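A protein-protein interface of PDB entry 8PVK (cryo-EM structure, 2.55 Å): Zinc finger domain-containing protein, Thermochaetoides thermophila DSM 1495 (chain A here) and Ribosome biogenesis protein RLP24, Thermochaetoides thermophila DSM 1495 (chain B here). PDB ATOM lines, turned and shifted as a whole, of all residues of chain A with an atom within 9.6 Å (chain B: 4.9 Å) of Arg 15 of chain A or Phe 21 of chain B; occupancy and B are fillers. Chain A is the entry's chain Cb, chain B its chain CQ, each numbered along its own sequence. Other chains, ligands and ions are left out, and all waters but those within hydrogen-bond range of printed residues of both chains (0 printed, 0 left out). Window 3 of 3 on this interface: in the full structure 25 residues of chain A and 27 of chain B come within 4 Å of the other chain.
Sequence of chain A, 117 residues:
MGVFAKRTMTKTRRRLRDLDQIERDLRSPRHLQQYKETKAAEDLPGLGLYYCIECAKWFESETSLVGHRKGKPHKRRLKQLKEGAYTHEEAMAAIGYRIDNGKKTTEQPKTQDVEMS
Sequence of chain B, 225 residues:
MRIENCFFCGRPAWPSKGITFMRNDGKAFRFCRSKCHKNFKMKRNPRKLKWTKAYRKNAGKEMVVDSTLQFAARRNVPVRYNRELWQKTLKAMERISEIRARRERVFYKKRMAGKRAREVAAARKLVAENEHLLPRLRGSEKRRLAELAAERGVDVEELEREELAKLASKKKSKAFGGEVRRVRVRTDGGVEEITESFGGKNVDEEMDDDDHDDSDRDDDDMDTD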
ATOM      1  N   THR A   8     -11.514 -16.237 -15.054  1.00  0.00           N
ATOM      2  CA  THR A   8     -11.515 -16.750 -13.690  1.00  0.00           C
ATOM      3  C   THR A   8     -10.120 -17.131 -13.202  1.00  0.00           C
ATOM      4  O   THR A   8      -9.974 -18.050 -12.394  1.00  0.00           O
ATOM      5  CB  THR A   8     -12.455 -17.950 -13.571  1.00  0.00           C
ATOM      6  OG1 THR A   8     -12.044 -18.978 -14.481  1.00  0.00           O
ATOM      7  CG2 THR A   8     -13.888 -17.542 -13.878  1.00  0.00           C
ATOM      8  N   MET A   9      -9.085 -16.430 -13.669  1.00  0.00           N
ATOM      9  CA  MET A   9      -7.729 -16.756 -13.243  1.00  0.00           C
ATOM     10  C   MET A   9      -7.416 -16.265 -11.834  1.00  0.00           C
ATOM     11  O   MET A   9      -6.425 -16.712 -11.248  1.00  0.00           O
ATOM     12  CB  MET A   9      -6.703 -16.182 -14.222  1.00  0.00           C
ATOM     13  CG  MET A   9      -6.654 -14.668 -14.279  1.00  0.00           C
ATOM     14  SD  MET A   9      -5.453 -14.088 -15.493  1.00  0.00           S
ATOM     15  CE  MET A   9      -5.638 -12.315 -15.341  1.00  0.00           C
ATOM     16  N   THR A  10      -8.227 -15.367 -11.282  1.00  0.00           N
ATOM     17  CA  THR A  10      -8.028 -14.874  -9.926  1.00  0.00           C
ATOM     18  C   THR A  10      -8.807 -15.665  -8.885  1.00  0.00           C
ATOM     19  O   THR A  10      -8.781 -15.300  -7.705  1.00  0.00           O
ATOM     20  CB  THR A  10      -8.409 -13.394  -9.834  1.00  0.00           C
ATOM     21  OG1 THR A  10      -9.644 -13.170 -10.524  1.00  0.00           O
ATOM     22  CG2 THR A  10      -7.324 -12.527 -10.445  1.00  0.00           C
ATOM     23  N   LYS A  11      -9.502 -16.725  -9.288  1.00  0.00           N
ATOM     24  CA  LYS A  11     -10.212 -17.570  -8.341  1.00  0.00           C
ATOM     25  C   LYS A  11      -9.227 -18.350  -7.477  1.00  0.00           C
ATOM     26  O   LYS A  11      -8.079 -18.588  -7.862  1.00  0.00           O
ATOM     27  CB  LYS A  11     -11.141 -18.535  -9.076  1.00  0.00           C
ATOM     28  CG  LYS A  11     -12.515 -17.973  -9.395  1.00  0.00           C
ATOM     29  CD  LYS A  11     -13.382 -19.015 -10.085  1.00  0.00           C
ATOM     30  CE  LYS A  11     -14.842 -18.600 -10.128  1.00  0.00           C
ATOM     31  NZ  LYS A  11     -15.516 -18.770  -8.817  1.00  0.00           N
ATOM     32  N   THR A  12      -9.692 -18.737  -6.286  1.00  0.00           N
ATOM     33  CA  THR A  12      -8.848 -19.478  -5.352  1.00  0.00           C
ATOM     34  C   THR A  12      -8.496 -20.859  -5.897  1.00  0.00           C
ATOM     35  O   THR A  12      -7.387 -21.359  -5.677  1.00  0.00           O
ATOM     36  CB  THR A  12      -9.553 -19.589  -3.999  1.00  0.00           C
ATOM     37  OG1 THR A  12     -10.019 -18.295  -3.598  1.00  0.00           O
ATOM     38  CG2 THR A  12      -8.608 -20.115  -2.938  1.00  0.00           C
ATOM     39  N   ARG A  13      -9.417 -21.481  -6.629  1.00  0.00           N
ATOM     40  CA  ARG A  13      -9.175 -22.791  -7.224  1.00  0.00           C
ATOM     41  C   ARG A  13      -8.282 -22.733  -8.459  1.00  0.00           C
ATOM     42  O   ARG A  13      -7.944 -23.789  -9.004  1.00  0.00           O
ATOM     43  CB  ARG A  13     -10.509 -23.463  -7.561  1.00  0.00           C
ATOM     44  CG  ARG A  13     -11.332 -22.755  -8.623  1.00  0.00           C
ATOM     45  CD  ARG A  13     -12.506 -23.616  -9.054  1.00  0.00           C
ATOM     46  NE  ARG A  13     -13.472 -22.871  -9.854  1.00  0.00           N
ATOM     47  CZ  ARG A  13     -13.421 -22.753 -11.174  1.00  0.00           C
ATOM     48  NH1 ARG A  13     -12.460 -23.321 -11.883  1.00  0.00           N
ATOM     49  NH2 ARG A  13     -14.360 -22.048 -11.798  1.00  0.00           N
ATOM     50  N   ARG A  14      -7.898 -21.539  -8.911  1.00  0.00           N
ATOM     51  CA  ARG A  14      -6.954 -21.362 -10.007  1.00  0.00           C
ATOM     52  C   ARG A  14      -5.627 -20.778  -9.531  1.00  0.00           C
ATOM     53  O   ARG A  14      -4.883 -20.202 -10.330  1.00  0.00           O
ATOM     54  CB  ARG A  14      -7.566 -20.473 -11.089  1.00  0.00           C
ATOM     55  CG  ARG A  14      -8.806 -21.055 -11.747  1.00  0.00           C
ATOM     56  CD  ARG A  14      -8.448 -21.884 -12.965  1.00  0.00           C
ATOM     57  NE  ARG A  14      -7.505 -21.189 -13.833  1.00  0.00           N
ATOM     58  CZ  ARG A  14      -7.854 -20.360 -14.808  1.00  0.00           C
ATOM     59  NH1 ARG A  14      -9.123 -20.094 -15.067  1.00  0.00           N
ATOM     60  NH2 ARG A  14      -6.905 -19.784 -15.539  1.00  0.00           N
ATOM     61  N   ARG A  15      -5.315 -20.922  -8.247  1.00  0.00           N
ATOM     62  CA  ARG A  15      -4.165 -20.268  -7.643  1.00  0.00           C
ATOM     63  C   ARG A  15      -2.876 -21.036  -7.926  1.00  0.00           C
ATOM     64  O   ARG A  15      -2.857 -22.268  -7.975  1.00  0.00           O
ATOM     65  CB  ARG A  15      -4.378 -20.136  -6.135  1.00  0.00           C
ATOM     66  CG  ARG A  15      -3.393 -19.241  -5.413  1.00  0.00           C
ATOM     67  CD  ARG A  15      -3.495 -19.448  -3.916  1.00  0.00           C
ATOM     68  NE  ARG A  15      -2.396 -18.816  -3.199  1.00  0.00           N
ATOM     69  CZ  ARG A  15      -1.233 -19.401  -2.952  1.00  0.00           C
ATOM     70  NH1 ARG A  15      -0.970 -20.626  -3.375  1.00  0.00           N
ATOM     71  NH2 ARG A  15      -0.314 -18.744  -2.252  1.00  0.00           N
ATOM     72  N   LEU A  16      -1.790 -20.288  -8.106  1.00  0.00           N
ATOM     73  CA  LEU A  16      -0.463 -20.836  -8.343  1.00  0.00           C
ATOM     74  C   LEU A  16       0.439 -20.573  -7.141  1.00  0.00           C
ATOM     75  O   LEU A  16       0.085 -19.845  -6.211  1.00  0.00           O
ATOM     76  CB  LEU A  16       0.149 -20.241  -9.617  1.00  0.00           C
ATOM     77  CG  LEU A  16      -0.707 -20.355 -10.882  1.00  0.00           C
ATOM     78  CD1 LEU A  16      -0.066 -19.604 -12.034  1.00  0.00           C
ATOM     79  CD2 LEU A  16      -0.932 -21.811 -11.248  1.00  0.00           C
ATOM     80  N   ARG A  17       1.621 -21.185  -7.175  1.00  0.00           N
ATOM     81  CA  ARG A  17       2.551 -21.118  -6.055  1.00  0.00           C
ATOM     82  C   ARG A  17       3.176 -19.731  -5.937  1.00  0.00           C
ATOM     83  O   ARG A  17       3.459 -19.071  -6.940  1.00  0.00           O
ATOM     84  CB  ARG A  17       3.640 -22.178  -6.220  1.00  0.00           C
ATOM     85  CG  ARG A  17       4.449 -22.457  -4.968  1.00  0.00           C
ATOM     86  CD  ARG A  17       5.037 -23.858  -5.006  1.00  0.00           C
ATOM     87  NE  ARG A  17       5.818 -24.161  -3.813  1.00  0.00           N
ATOM     88  CZ  ARG A  17       5.299 -24.552  -2.657  1.00  0.00           C
ATOM     89  NH1 ARG A  17       3.994 -24.689  -2.495  1.00  0.00           N
ATOM     90  NH2 ARG A  17       6.111 -24.813  -1.638  1.00  0.00           N
ATOM     91  N   ASP A  18       3.397 -19.294  -4.697  1.00  0.00           N
ATOM     92  CA  ASP A  18       3.938 -17.971  -4.424  1.00  0.00           C
ATOM     93  C   ASP A  18       5.463 -17.953  -4.509  1.00  0.00           C
ATOM     94  O   ASP A  18       6.141 -18.976  -4.372  1.00  0.00           O
ATOM     95  CB  ASP A  18       3.500 -17.480  -3.046  1.00  0.00           C
ATOM     96  CG  ASP A  18       2.097 -16.920  -3.044  1.00  0.00           C
ATOM     97  OD1 ASP A  18       1.482 -16.856  -4.126  1.00  0.00           O
ATOM     98  OD2 ASP A  18       1.606 -16.546  -1.959  1.00  0.00           O
ATOM     99  N   LEU A  19       5.996 -16.743  -4.709  1.00  0.00           N
ATOM    100  CA  LEU A  19       7.423 -16.567  -4.948  1.00  0.00           C
ATOM    101  C   LEU A  19       8.258 -16.837  -3.701  1.00  0.00           C
ATOM    102  O   LEU A  19       9.374 -17.355  -3.813  1.00  0.00           O
ATOM    103  CB  LEU A  19       7.692 -15.157  -5.470  1.00  0.00           C
ATOM    104  CG  LEU A  19       8.972 -14.972  -6.282  1.00  0.00           C
ATOM    105  CD1 LEU A  19       8.904 -15.782  -7.565  1.00  0.00           C
ATOM    106  CD2 LEU A  19       9.205 -13.503  -6.583  1.00  0.00           C
ATOM    107  N   ASP A  20       7.756 -16.489  -2.513  1.00  0.00           N
ATOM    108  CA  ASP A  20       8.496 -16.810  -1.295  1.00  0.00           C
ATOM    109  C   ASP A  20       8.514 -18.312  -1.035  1.00  0.00           C
ATOM    110  O   ASP A  20       9.519 -18.847  -0.546  1.00  0.00           O
ATOM    111  CB  ASP A  20       7.908 -16.060  -0.099  1.00  0.00           C
ATOM    112  CG  ASP A  20       6.407 -16.227   0.019  1.00  0.00           C
ATOM    113  OD1 ASP A  20       5.808 -16.885  -0.852  1.00  0.00           O
ATOM    114  OD2 ASP A  20       5.825 -15.695   0.988  1.00  0.00           O
ATOM    115  N   GLN A  21       7.422 -19.004  -1.369  1.00  0.00           N
ATOM    116  CA  GLN A  21       7.418 -20.460  -1.306  1.00  0.00           C
ATOM    117  C   GLN A  21       8.409 -21.050  -2.299  1.00  0.00           C
ATOM    118  O   GLN A  21       9.068 -22.051  -2.006  1.00  0.00           O
ATOM    119  CB  GLN A  21       6.012 -20.996  -1.565  1.00  0.00           C
ATOM    120  CG  GLN A  21       4.946 -20.397  -0.668  1.00  0.00           C
ATOM    121  CD  GLN A  21       3.569 -20.963  -0.946  1.00  0.00           C
ATOM    122  OE1 GLN A  21       2.942 -20.636  -1.953  1.00  0.00           O
ATOM    123  NE2 GLN A  21       3.095 -21.824  -0.056  1.00  0.00           N
ATOM    124  N   ILE A  22       8.541 -20.428  -3.473  1.00  0.00           N
ATOM    125  CA  ILE A  22       9.525 -20.884  -4.453  1.00  0.00           C
ATOM    126  C   ILE A  22      10.951 -20.646  -3.948  1.00  0.00           C
ATOM    127  O   ILE A  22      11.839 -21.486  -4.147  1.00  0.00           O
ATOM    128  CB  ILE A  22       9.253 -20.208  -5.812  1.00  0.00           C
ATOM    129  CG1 ILE A  22       7.978 -20.784  -6.431  1.00  0.00           C
ATOM    130  CG2 ILE A  22      10.412 -20.385  -6.777  1.00  0.00           C
ATOM    131  CD1 ILE A  22       7.264 -19.841  -7.363  1.00  0.00           C
ATOM    132  N   ARG A  24      11.863 -20.615  -0.728  1.00  0.00           N
ATOM    133  CA  ARG A  24      12.102 -21.633   0.291  1.00  0.00           C
ATOM    134  C   ARG A  24      12.259 -23.021  -0.323  1.00  0.00           C
ATOM    135  O   ARG A  24      12.980 -23.860   0.228  1.00  0.00           O
ATOM    136  CB  ARG A  24      10.978 -21.626   1.327  1.00  0.00           C
ATOM    137  CG  ARG A  24      11.236 -20.698   2.508  1.00  0.00           C
ATOM    138  CD  ARG A  24      10.258 -20.960   3.654  1.00  0.00           C
ATOM    139  NE  ARG A  24       8.861 -20.730   3.293  1.00  0.00           N
ATOM    140  CZ  ARG A  24       8.317 -19.544   3.050  1.00  0.00           C
ATOM    141  NH1 ARG A  24       9.007 -18.422   3.188  1.00  0.00           N
ATOM    142  NH2 ARG A  24       7.040 -19.479   2.687  1.00  0.00           N
ATOM    143  N   TYR A  35       6.098 -30.077  -0.789  1.00  0.00           N
ATOM    144  CA  TYR A  35       5.216 -29.683  -1.885  1.00  0.00           C
ATOM    145  C   TYR A  35       5.005 -30.819  -2.878  1.00  0.00           C
ATOM    146  O   TYR A  35       3.911 -30.959  -3.434  1.00  0.00           O
ATOM    147  CB  TYR A  35       5.767 -28.453  -2.607  1.00  0.00           C
ATOM    148  CG  TYR A  35       4.929 -28.028  -3.797  1.00  0.00           C
ATOM    149  CD1 TYR A  35       3.574 -27.755  -3.651  1.00  0.00           C
ATOM    150  CD2 TYR A  35       5.489 -27.901  -5.063  1.00  0.00           C
ATOM    151  CE1 TYR A  35       2.799 -27.367  -4.732  1.00  0.00           C
ATOM    152  CE2 TYR A  35       4.721 -27.511  -6.150  1.00  0.00           C
ATOM    153  CZ  TYR A  35       3.376 -27.246  -5.977  1.00  0.00           C
ATOM    154  OH  TYR A  35       2.606 -26.859  -7.050  1.00  0.00           O
ATOM    155  N   LYS A  39       1.384 -33.830  -4.034  1.00  0.00           N
ATOM    156  CA  LYS A  39       0.878 -34.144  -5.363  1.00  0.00           C
ATOM    157  C   LYS A  39       1.042 -35.633  -5.637  1.00  0.00           C
ATOM    158  O   LYS A  39       1.771 -36.340  -4.936  1.00  0.00           O
ATOM    159  CB  LYS A  39       1.598 -33.331  -6.450  1.00  0.00           C
ATOM    160  CG  LYS A  39       1.452 -31.827  -6.306  1.00  0.00           C
ATOM    161  CD  LYS A  39       0.008 -31.404  -6.507  1.00  0.00           C
ATOM    162  CE  LYS A  39      -0.130 -29.892  -6.533  1.00  0.00           C
ATOM    163  NZ  LYS A  39       0.135 -29.294  -5.197  1.00  0.00           N
ATOM    164  N   ALA A  56       7.966 -23.338 -10.809  1.00  0.00           N
ATOM    165  CA  ALA A  56       7.131 -24.220  -9.981  1.00  0.00           C
ATOM    166  C   ALA A  56       6.176 -25.048 -10.835  1.00  0.00           C
ATOM    167  O   ALA A  56       4.998 -25.208 -10.509  1.00  0.00           O
ATOM    168  CB  ALA A  56       6.365 -23.431  -8.915  1.00  0.00           C
ATOM    169  N   ARG A  77      10.791 -14.981 -14.046  1.00  0.00           N
ATOM    170  CA  ARG A  77      10.866 -15.606 -12.731  1.00  0.00           C
ATOM    171  C   ARG A  77      12.269 -15.496 -12.146  1.00  0.00           C
ATOM    172  O   ARG A  77      12.428 -15.252 -10.944  1.00  0.00           O
ATOM    173  CB  ARG A  77      10.432 -17.068 -12.822  1.00  0.00           C
ATOM    174  CG  ARG A  77       8.951 -17.284 -12.580  1.00  0.00           C
ATOM    175  CD  ARG A  77       8.554 -16.867 -11.173  1.00  0.00           C
ATOM    176  NE  ARG A  77       7.107 -16.835 -10.998  1.00  0.00           N
ATOM    177  CZ  ARG A  77       6.358 -17.896 -10.737  1.00  0.00           C
ATOM    178  NH1 ARG A  77       6.882 -19.106 -10.631  1.00  0.00           N
ATOM    179  NH2 ARG A  77       5.046 -17.742 -10.584  1.00  0.00           N
ATOM    180  N   HIS A  88       7.157 -11.350   5.309  1.00  0.00           N
ATOM    181  CA  HIS A  88       6.698 -10.685   6.524  1.00  0.00           C
ATOM    182  C   HIS A  88       7.819  -9.916   7.208  1.00  0.00           C
ATOM    183  O   HIS A  88       7.558  -8.895   7.854  1.00  0.00           O
ATOM    184  CB  HIS A  88       6.099 -11.704   7.493  1.00  0.00           C
ATOM    185  CG  HIS A  88       4.659 -12.017   7.228  1.00  0.00           C
ATOM    186  ND1 HIS A  88       4.260 -13.104   6.482  1.00  0.00           N
ATOM    187  CD2 HIS A  88       3.525 -11.390   7.617  1.00  0.00           C
ATOM    188  CE1 HIS A  88       2.942 -13.131   6.418  1.00  0.00           C
ATOM    189  NE2 HIS A  88       2.471 -12.101   7.098  1.00  0.00           N
ATOM    190  N   ILE B  19      -9.318  -8.458   5.272  1.00  0.00           N
ATOM    191  CA  ILE B  19      -9.495  -9.902   5.199  1.00  0.00           C
ATOM    192  C   ILE B  19      -8.141 -10.570   5.403  1.00  0.00           C
ATOM    193  O   ILE B  19      -7.089  -9.968   5.175  1.00  0.00           O
ATOM    194  CB  ILE B  19     -10.153 -10.315   3.855  1.00  0.00           C
ATOM    195  CG1 ILE B  19     -10.862 -11.664   3.979  1.00  0.00           C
ATOM    196  CG2 ILE B  19      -9.136 -10.341   2.718  1.00  0.00           C
ATOM    197  CD1 ILE B  19     -11.696 -12.024   2.777  1.00  0.00           C
ATOM    198  N   THR B  20      -8.167 -11.817   5.859  1.00  0.00           N
ATOM    199  CA  THR B  20      -6.951 -12.577   6.102  1.00  0.00           C
ATOM    200  C   THR B  20      -6.925 -13.813   5.214  1.00  0.00           C
ATOM    201  O   THR B  20      -7.913 -14.547   5.131  1.00  0.00           O
ATOM    202  CB  THR B  20      -6.838 -12.981   7.572  1.00  0.00           C
ATOM    203  OG1 THR B  20      -7.150 -11.855   8.398  1.00  0.00           O
ATOM    204  CG2 THR B  20      -5.419 -13.409   7.872  1.00  0.00           C
ATOM    205  N   PHE B  21      -5.792 -14.036   4.559  1.00  0.00           N
ATOM    206  CA  PHE B  21      -5.571 -15.206   3.723  1.00  0.00           C
ATOM    207  C   PHE B  21      -4.756 -16.219   4.519  1.00  0.00           C
ATOM    208  O   PHE B  21      -3.683 -15.890   5.035  1.00  0.00           O
ATOM    209  CB  PHE B  21      -4.852 -14.817   2.432  1.00  0.00           C
ATOM    210  CG  PHE B  21      -4.380 -15.987   1.619  1.00  0.00           C
ATOM    211  CD1 PHE B  21      -5.248 -17.017   1.291  1.00  0.00           C
ATOM    212  CD2 PHE B  21      -3.070 -16.051   1.170  1.00  0.00           C
ATOM    213  CE1 PHE B  21      -4.818 -18.090   0.541  1.00  0.00           C
ATOM    214  CE2 PHE B  21      -2.636 -17.123   0.417  1.00  0.00           C
ATOM    215  CZ  PHE B  21      -3.510 -18.143   0.102  1.00  0.00           C
ATOM    216  N   MET B  22      -5.268 -17.442   4.617  1.00  0.00           N
ATOM    217  CA  MET B  22      -4.654 -18.504   5.406  1.00  0.00           C
ATOM    218  C   MET B  22      -4.019 -19.491   4.432  1.00  0.00           C
ATOM    219  O   MET B  22      -4.731 -20.185   3.699  1.00  0.00           O
ATOM    220  CB  MET B  22      -5.708 -19.198   6.267  1.00  0.00           C
ATOM    221  CG  MET B  22      -6.348 -18.351   7.369  1.00  0.00           C
ATOM    222  SD  MET B  22      -5.456 -18.224   8.924  1.00  0.00           S
ATOM    223  CE  MET B  22      -5.947 -16.608   9.498  1.00  0.00           C
ATOM    224  N   ARG B  23      -2.689 -19.568   4.418  1.00  0.00           N
ATOM    225  CA  ARG B  23      -1.981 -20.422   3.476  1.00  0.00           C
ATOM    226  C   ARG B  23      -1.714 -21.792   4.092  1.00  0.00           C
ATOM    227  O   ARG B  23      -1.606 -21.934   5.312  1.00  0.00           O
ATOM    228  CB  ARG B  23      -0.665 -19.774   3.038  1.00  0.00           C
ATOM    229  CG  ARG B  23      -0.230 -20.165   1.637  1.00  0.00           C
ATOM    230  CD  ARG B  23       0.654 -19.107   0.997  1.00  0.00           C
ATOM    231  NE  ARG B  23       1.967 -19.018   1.623  1.00  0.00           N
ATOM    232  CZ  ARG B  23       2.884 -18.114   1.308  1.00  0.00           C
ATOM    233  NH1 ARG B  23       2.666 -17.204   0.373  1.00  0.00           N
ATOM    234  NH2 ARG B  23       4.052 -18.125   1.945  1.00  0.00           N
ATOM    235  N   LYS B  27       0.999 -19.801   7.069  1.00  0.00           N
ATOM    236  CA  LYS B  27       1.189 -18.359   7.143  1.00  0.00           C
ATOM    237  C   LYS B  27      -0.132 -17.624   6.961  1.00  0.00           C
ATOM    238  O   LYS B  27      -0.923 -17.949   6.069  1.00  0.00           O
ATOM    239  CB  LYS B  27       2.192 -17.875   6.092  1.00  0.00           C
ATOM    240  CG  LYS B  27       3.591 -18.426   6.262  1.00  0.00           C
ATOM    241  CD  LYS B  27       4.199 -17.940   7.568  1.00  0.00           C
ATOM    242  CE  LYS B  27       4.525 -16.458   7.504  1.00  0.00           C
ATOM    243  NZ  LYS B  27       5.193 -15.981   8.747  1.00  0.00           N
ATOM    244  N   ALA B  28      -0.361 -16.627   7.808  1.00  0.00           N
ATOM    245  CA  ALA B  28      -1.518 -15.754   7.697  1.00  0.00           C
ATOM    246  C   ALA B  28      -1.100 -14.408   7.118  1.00  0.00           C
ATOM    247  O   ALA B  28      -0.077 -13.837   7.502  1.00  0.00           O
ATOM    248  CB  ALA B  28      -2.187 -15.557   9.059  1.00  0.00           C
ATOM    249  N   PHE B  29      -1.904 -13.909   6.184  1.00  0.00           N
ATOM    250  CA  PHE B  29      -1.642 -12.642   5.514  1.00  0.00           C
ATOM    251  C   PHE B  29      -2.828 -11.724   5.755  1.00  0.00           C
ATOM    252  O   PHE B  29      -3.925 -11.989   5.260  1.00  0.00           O
ATOM    253  CB  PHE B  29      -1.426 -12.844   4.012  1.00  0.00           C
ATOM    254  CG  PHE B  29      -0.225 -13.676   3.675  1.00  0.00           C
ATOM    255  CD1 PHE B  29      -0.325 -15.054   3.577  1.00  0.00           C
ATOM    256  CD2 PHE B  29       1.004 -13.081   3.449  1.00  0.00           C
ATOM    257  CE1 PHE B  29       0.778 -15.823   3.266  1.00  0.00           C
ATOM    258  CE2 PHE B  29       2.112 -13.844   3.137  1.00  0.00           C
ATOM    259  CZ  PHE B  29       1.998 -15.216   3.047  1.00  0.00           C
ATOM    260  N   PHE B  31      -4.777  -8.247   5.263  1.00  0.00           N
ATOM    261  CA  PHE B  31      -4.923  -7.129   4.348  1.00  0.00           C
ATOM    262  C   PHE B  31      -5.974  -6.184   4.898  1.00  0.00           C
ATOM    263  O   PHE B  31      -7.044  -6.622   5.334  1.00  0.00           O
ATOM    264  CB  PHE B  31      -5.330  -7.600   2.951  1.00  0.00           C
ATOM    265  CG  PHE B  31      -4.458  -8.685   2.409  1.00  0.00           C
ATOM    266  CD1 PHE B  31      -3.216  -8.389   1.874  1.00  0.00           C
ATOM    267  CD2 PHE B  31      -4.871 -10.005   2.451  1.00  0.00           C
ATOM    268  CE1 PHE B  31      -2.409  -9.390   1.384  1.00  0.00           C
ATOM    269  CE2 PHE B  31      -4.067 -11.010   1.963  1.00  0.00           C
ATOM    270  CZ  PHE B  31      -2.835 -10.703   1.431  1.00  0.00           C
ATOM    271  N   PHE B  40      -2.652  -8.594  -4.121  1.00  0.00           N
ATOM    272  CA  PHE B  40      -1.995  -9.827  -3.692  1.00  0.00           C
ATOM    273  C   PHE B  40      -2.456 -11.025  -4.518  1.00  0.00           C
ATOM    274  O   PHE B  40      -1.647 -11.887  -4.877  1.00  0.00           O
ATOM    275  CB  PHE B  40      -2.260 -10.057  -2.205  1.00  0.00           C
ATOM    276  CG  PHE B  40      -1.587 -11.277  -1.642  1.00  0.00           C
ATOM    277  CD1 PHE B  40      -0.276 -11.218  -1.202  1.00  0.00           C
ATOM    278  CD2 PHE B  40      -2.277 -12.475  -1.520  1.00  0.00           C
ATOM    279  CE1 PHE B  40       0.341 -12.335  -0.675  1.00  0.00           C
ATOM    280  CE2 PHE B  40      -1.665 -13.593  -0.998  1.00  0.00           C
ATOM    281  CZ  PHE B  40      -0.354 -13.523  -0.572  1.00  0.00           C
ATOM    282  N   LYS B  43      -0.833 -11.060  -7.596  1.00  0.00           N
ATOM    283  CA  LYS B  43       0.600 -11.307  -7.378  1.00  0.00           C
ATOM    284  C   LYS B  43       1.441 -10.097  -7.782  1.00  0.00           C
ATOM    285  O   LYS B  43       2.495 -10.236  -8.402  1.00  0.00           O
ATOM    286  CB  LYS B  43       1.103 -12.570  -8.097  1.00  0.00           C
ATOM    287  CG  LYS B  43       0.179 -13.785  -8.061  1.00  0.00           C
ATOM    288  CD  LYS B  43       0.342 -14.613  -6.805  1.00  0.00           C
ATOM    289  CE  LYS B  43      -0.402 -15.932  -6.951  1.00  0.00           C
ATOM    290  NZ  LYS B  43      -0.140 -16.872  -5.833  1.00  0.00           N
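The side-chain amino group (NZ) of Lys 43 of chain B lies close to the side-chain carboxylate (OD1) of Asp 18 of chain A (2.4 Å).
The backbone carbonyl oxygen of Leu 16 of chain A is in hydrogen-bond range of the side-chain amino group of Lys 43 of chain B, at 3.0 Å.
NE of Arg 23 of chain B lies close to NE2 of Gln 21 of chain A (3.5 Å).
A ring nitrogen (NE2) of His 88 of chain A is in hydrogen-bond range of the backbone carbonyl oxygen (O) of Ala 28 of chain B (3.1 Å).
NH2 of Arg 23 of chain B lies within salt-bridge range of OD2 of Asp 20 of chain A (3.2 Å).
NH1 of Arg 23 of chain B is in salt-bridge range of OD2 of Asp 18 of chain A (2.6 Å).
The guanidinium group (NH2) of Arg 24 of chain A lies close to the guanidinium group (NH2) of Arg 23 of chain B, 3.4 Å away.
The backbone NH (N) of Phe 21 of chain B sits at hydrogen-bond distance from the backbone carbonyl oxygen (O) of Phe 29 of chain B.
OE1 of Gln 21 of chain A lies within hydrogen-bond range of N of Asp 18 of chain A (3.1 Å).
The side-chain carboxylate (OD2) of Asp 18 of chain A lies within salt-bridge range of the guanidinium group (NH2) of Arg 15 of chain A, 2.9 Å away.
Among the printed residues, pairs that only touch across the chains: Arg 15 of chain A with Phe 21 of chain B (3.5 Å), Arg 15 of chain A with Arg 23 of chain B (3.4 Å), Arg 15 of chain A with Lys 43 of chain B (3.98 Å), Asp 18 of chain A with Phe 40 of chain B (3.9 Å), His 88 of chain A with Lys 27 of chain B (3.5 Å) and His 88 of chain A with Phe 29 of chain B (3.5 Å).
Arg 15 of chain A touches just these residues of chain B: Phe 21 (3.5 Å), Arg 23 (3.4 Å) and Lys 43 (3.98 Å).
Of the printed residues of chain B, Asp 18 of chain A touches Arg 23, Phe 40 and Lys 43.
Printed residues of chain B within 4 Å of Arg 24 of chain A: Arg 23.
Phe 21 of chain B touches one residue of chain A.
Printed residues of chain A within 4 Å of Arg 23 of chain B: Arg 15 (3.4 Å), Asp 18 (2.6 Å), Asp 20 (3.2 Å), Gln 21 (3.5 Å) and Arg 24 (3.4 Å).
The nearest residue of chain A that does not touch Phe 21 of chain B is Asp 18 of chain A (4.9 Å).
Printed residues of chain A that touch a printed residue of chain B: Arg 15, Leu 16, Asp 18, Asp 20, Gln 21, Arg 24 and His 88.
Hydrophobic or aromatic side chains of chain A that line the printed part of chain B: His 88.
Among the printed residues, Asp or Glu carboxylates within 4 Å of a Lys or Arg side-chain nitrogen of the other chain: Asp 18 of chain A with Arg 23 of chain B, Asp 18 of chain A with Lys 43 of chain B and Asp 20 of chain A with Arg 23 of chain B.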
